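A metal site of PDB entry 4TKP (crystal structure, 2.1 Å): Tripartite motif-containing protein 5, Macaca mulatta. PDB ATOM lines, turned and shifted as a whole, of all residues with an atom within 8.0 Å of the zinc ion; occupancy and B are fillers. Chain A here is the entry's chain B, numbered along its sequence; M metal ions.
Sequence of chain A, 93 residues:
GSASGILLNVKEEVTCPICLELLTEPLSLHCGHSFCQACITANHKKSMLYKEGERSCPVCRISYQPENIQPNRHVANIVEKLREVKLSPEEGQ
SG of Cys 36 lies close to N of Thr 24, 3.3 Å away. SG of Cys 16 sits close to N of Ile 18 (3.5 Å). N of Glu 21 sits close to SG of Cys 19 (3.3 Å). The backbone NH of Cys 16 sits at hydrogen-bond distance from the backbone carbonyl oxygen of Glu 21.
Four residues have an atom within 4 Å of the zinc ion: Cys 16, Cys 19, Cys 36 and Cys 39. The nearest printed residue that does not touch the zinc ion is Ile 18 (4.5 Å).
The side-chain sulfur (SG) of Cys 19 binds the zinc ion (2.3 Å). The zinc ion is bound by SG of Cys 39, at 2.3 Å. The zinc ion is bound by the side-chain sulfur (SG) of Cys 16 (2.5 Å). SG of Cys 36 is bound to the zinc ion, 2.8 Å away.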
ATOM      1  N   THR A  15       6.988  19.535 -23.746  1.00  0.00           N
ATOM      2  CA  THR A  15       5.613  19.488 -24.244  1.00  0.00           C
ATOM      3  C   THR A  15       4.684  18.982 -23.155  1.00  0.00           C
ATOM      4  O   THR A  15       4.942  17.954 -22.535  1.00  0.00           O
ATOM      5  CB  THR A  15       5.495  18.574 -25.480  1.00  0.00           C
ATOM      6  OG1 THR A  15       6.227  19.142 -26.579  1.00  0.00           O
ATOM      7  CG2 THR A  15       4.027  18.414 -25.890  1.00  0.00           C
ATOM      8  N   CYS A  16       3.604  19.712 -22.917  1.00  0.00           N
ATOM      9  CA  CYS A  16       2.581  19.297 -21.962  1.00  0.00           C
ATOM     10  C   CYS A  16       1.865  18.053 -22.473  1.00  0.00           C
ATOM     11  O   CYS A  16       1.253  18.084 -23.536  1.00  0.00           O
ATOM     12  CB  CYS A  16       1.578  20.425 -21.731  1.00  0.00           C
ATOM     13  SG  CYS A  16       0.212  19.996 -20.628  1.00  0.00           S
ATOM     14  N   PRO A  17       1.925  16.962 -21.705  1.00  0.00           N
ATOM     15  CA  PRO A  17       1.318  15.686 -22.125  1.00  0.00           C
ATOM     16  C   PRO A  17      -0.215  15.721 -22.166  1.00  0.00           C
ATOM     17  O   PRO A  17      -0.822  14.759 -22.621  1.00  0.00           O
ATOM     18  CB  PRO A  17       1.802  14.693 -21.059  1.00  0.00           C
ATOM     19  CG  PRO A  17       2.117  15.532 -19.872  1.00  0.00           C
ATOM     20  CD  PRO A  17       2.628  16.834 -20.411  1.00  0.00           C
ATOM     21  N   ILE A  18      -0.815  16.814 -21.717  1.00  0.00           N
ATOM     22  CA  ILE A  18      -2.273  16.939 -21.739  1.00  0.00           C
ATOM     23  C   ILE A  18      -2.773  17.639 -23.001  1.00  0.00           C
ATOM     24  O   ILE A  18      -3.508  17.062 -23.784  1.00  0.00           O
ATOM     25  CB  ILE A  18      -2.798  17.691 -20.505  1.00  0.00           C
ATOM     26  CG1 ILE A  18      -2.338  16.985 -19.218  1.00  0.00           C
ATOM     27  CG2 ILE A  18      -4.315  17.782 -20.544  1.00  0.00           C
ATOM     28  CD1 ILE A  18      -2.765  15.541 -19.135  1.00  0.00           C
ATOM     29  N   CYS A  19      -2.363  18.891 -23.183  1.00  0.00           N
ATOM     30  CA  CYS A  19      -2.813  19.673 -24.329  1.00  0.00           C
ATOM     31  C   CYS A  19      -1.940  19.422 -25.561  1.00  0.00           C
ATOM     32  O   CYS A  19      -2.297  19.790 -26.680  1.00  0.00           O
ATOM     33  CB  CYS A  19      -2.796  21.163 -23.991  1.00  0.00           C
ATOM     34  SG  CYS A  19      -1.135  21.875 -23.873  1.00  0.00           S
ATOM     35  N   LEU A  20      -0.781  18.788 -25.330  1.00  0.00           N
ATOM     36  CA  LEU A  20       0.188  18.502 -26.386  1.00  0.00           C
ATOM     37  C   LEU A  20       0.736  19.750 -27.066  1.00  0.00           C
ATOM     38  O   LEU A  20       1.165  19.706 -28.228  1.00  0.00           O
ATOM     39  CB  LEU A  20      -0.385  17.509 -27.410  1.00  0.00           C
ATOM     40  CG  LEU A  20      -0.703  16.134 -26.832  1.00  0.00           C
ATOM     41  CD1 LEU A  20      -1.092  15.172 -27.938  1.00  0.00           C
ATOM     42  CD2 LEU A  20       0.470  15.596 -26.028  1.00  0.00           C
ATOM     43  N   GLU A  21       0.742  20.858 -26.335  1.00  0.00           N
ATOM     44  CA  GLU A  21       1.400  22.083 -26.784  1.00  0.00           C
ATOM     45  C   GLU A  21       2.567  22.386 -25.870  1.00  0.00           C
ATOM     46  O   GLU A  21       2.721  21.759 -24.817  1.00  0.00           O
ATOM     47  CB  GLU A  21       0.418  23.261 -26.803  1.00  0.00           C
ATOM     48  CG  GLU A  21      -0.381  23.366 -28.090  1.00  0.00           C
ATOM     49  CD  GLU A  21       0.492  23.727 -29.278  1.00  0.00           C
ATOM     50  OE1 GLU A  21       1.414  24.553 -29.113  1.00  0.00           O
ATOM     51  OE2 GLU A  21       0.250  23.176 -30.376  1.00  0.00           O
ATOM     52  N   LEU A  22       3.402  23.349 -26.265  1.00  0.00           N
ATOM     53  CA  LEU A  22       4.518  23.769 -25.436  1.00  0.00           C
ATOM     54  C   LEU A  22       4.023  24.256 -24.086  1.00  0.00           C
ATOM     55  O   LEU A  22       2.997  24.935 -24.014  1.00  0.00           O
ATOM     56  CB  LEU A  22       5.332  24.869 -26.138  1.00  0.00           C
ATOM     57  CG  LEU A  22       6.113  24.449 -27.382  1.00  0.00           C
ATOM     58  CD1 LEU A  22       6.974  25.592 -27.885  1.00  0.00           C
ATOM     59  CD2 LEU A  22       6.952  23.213 -27.094  1.00  0.00           C
ATOM     60  N   LEU A  23       4.739  23.896 -23.034  1.00  0.00           N
ATOM     61  CA  LEU A  23       4.352  24.240 -21.662  1.00  0.00           C
ATOM     62  C   LEU A  23       4.113  25.740 -21.477  1.00  0.00           C
ATOM     63  O   LEU A  23       4.948  26.563 -21.849  1.00  0.00           O
ATOM     64  CB  LEU A  23       5.417  23.755 -20.673  1.00  0.00           C
ATOM     65  CG  LEU A  23       5.523  22.234 -20.490  1.00  0.00           C
ATOM     66  CD1 LEU A  23       6.843  21.871 -19.835  1.00  0.00           C
ATOM     67  CD2 LEU A  23       4.366  21.725 -19.663  1.00  0.00           C
ATOM     68  N   THR A  24       2.956  26.077 -20.920  1.00  0.00           N
ATOM     69  CA  THR A  24       2.617  27.453 -20.603  1.00  0.00           C
ATOM     70  C   THR A  24       2.346  27.568 -19.111  1.00  0.00           C
ATOM     71  O   THR A  24       1.430  26.939 -18.592  1.00  0.00           O
ATOM     72  CB  THR A  24       1.394  27.928 -21.398  1.00  0.00           C
ATOM     73  OG1 THR A  24       1.730  28.021 -22.784  1.00  0.00           O
ATOM     74  CG2 THR A  24       0.936  29.293 -20.904  1.00  0.00           C
ATOM     75  N   SER A  34       5.946  17.840 -15.671  1.00  0.00           N
ATOM     76  CA  SER A  34       5.375  19.173 -15.608  1.00  0.00           C
ATOM     77  C   SER A  34       4.198  19.336 -16.569  1.00  0.00           C
ATOM     78  O   SER A  34       4.093  18.634 -17.567  1.00  0.00           O
ATOM     79  CB  SER A  34       6.438  20.228 -15.911  1.00  0.00           C
ATOM     80  OG  SER A  34       7.591  20.024 -15.112  1.00  0.00           O
ATOM     81  N   PHE A  35       3.318  20.278 -16.249  1.00  0.00           N
ATOM     82  CA  PHE A  35       2.114  20.524 -17.037  1.00  0.00           C
ATOM     83  C   PHE A  35       1.838  22.012 -17.102  1.00  0.00           C
ATOM     84  O   PHE A  35       2.312  22.771 -16.261  1.00  0.00           O
ATOM     85  CB  PHE A  35       0.904  19.810 -16.401  1.00  0.00           C
ATOM     86  CG  PHE A  35       1.161  18.363 -16.068  1.00  0.00           C
ATOM     87  CD1 PHE A  35       1.753  17.999 -14.871  1.00  0.00           C
ATOM     88  CD2 PHE A  35       0.783  17.369 -16.952  1.00  0.00           C
ATOM     89  CE1 PHE A  35       1.985  16.678 -14.569  1.00  0.00           C
ATOM     90  CE2 PHE A  35       1.007  16.037 -16.645  1.00  0.00           C
ATOM     91  CZ  PHE A  35       1.601  15.696 -15.456  1.00  0.00           C
ATOM     92  N   CYS A  36       1.069  22.439 -18.101  1.00  0.00           N
ATOM     93  CA  CYS A  36       0.608  23.813 -18.168  1.00  0.00           C
ATOM     94  C   CYS A  36      -0.249  24.086 -16.948  1.00  0.00           C
ATOM     95  O   CYS A  36      -0.971  23.202 -16.483  1.00  0.00           O
ATOM     96  CB  CYS A  36      -0.218  24.062 -19.436  1.00  0.00           C
ATOM     97  SG  CYS A  36       0.662  23.757 -20.991  1.00  0.00           S
ATOM     98  N   GLN A  37      -0.178  25.304 -16.403  1.00  0.00           N
ATOM     99  CA  GLN A  37      -0.918  25.648 -15.193  1.00  0.00           C
ATOM    100  C   GLN A  37      -2.423  25.478 -15.383  1.00  0.00           C
ATOM    101  O   GLN A  37      -3.144  25.133 -14.459  1.00  0.00           O
ATOM    102  CB  GLN A  37      -0.572  27.071 -14.727  1.00  0.00           C
ATOM    103  CG  GLN A  37      -1.672  28.105 -14.911  1.00  0.00           C
ATOM    104  CD  GLN A  37      -2.624  28.186 -13.731  1.00  0.00           C
ATOM    105  OE1 GLN A  37      -2.580  27.350 -12.829  1.00  0.00           O
ATOM    106  NE2 GLN A  37      -3.484  29.197 -13.722  1.00  0.00           N
ATOM    107  N   ALA A  38      -2.889  25.697 -16.611  1.00  0.00           N
ATOM    108  CA  ALA A  38      -4.305  25.565 -16.932  1.00  0.00           C
ATOM    109  C   ALA A  38      -4.715  24.110 -17.044  1.00  0.00           C
ATOM    110  O   ALA A  38      -5.900  23.785 -16.984  1.00  0.00           O
ATOM    111  CB  ALA A  38      -4.627  26.316 -18.212  1.00  0.00           C
ATOM    112  N   CYS A  39      -3.727  23.220 -17.190  1.00  0.00           N
ATOM    113  CA  CYS A  39      -4.006  21.814 -17.440  1.00  0.00           C
ATOM    114  C   CYS A  39      -4.142  20.975 -16.164  1.00  0.00           C
ATOM    115  O   CYS A  39      -4.412  19.775 -16.231  1.00  0.00           O
ATOM    116  CB  CYS A  39      -2.946  21.215 -18.372  1.00  0.00           C
ATOM    117  SG  CYS A  39      -3.021  21.867 -20.057  1.00  0.00           S
ATOM    118  N   ILE A  40      -3.944  21.597 -15.010  1.00  0.00           N
ATOM    119  CA  ILE A  40      -4.243  20.943 -13.733  1.00  0.00           C
ATOM    120  C   ILE A  40      -5.007  21.880 -12.798  1.00  0.00           C
ATOM    121  O   ILE A  40      -4.434  22.767 -12.171  1.00  0.00           O
ATOM    122  CB  ILE A  40      -2.973  20.442 -13.011  1.00  0.00           C
ATOM    123  CG1 ILE A  40      -2.205  19.441 -13.880  1.00  0.00           C
ATOM    124  CG2 ILE A  40      -3.340  19.792 -11.674  1.00  0.00           C
ATOM    125  CD1 ILE A  40      -1.141  18.678 -13.128  1.00  0.00           C
HETATM  126 ZN    ZN M   1      -1.211  21.808 -21.543  1.00  0.00          ZN
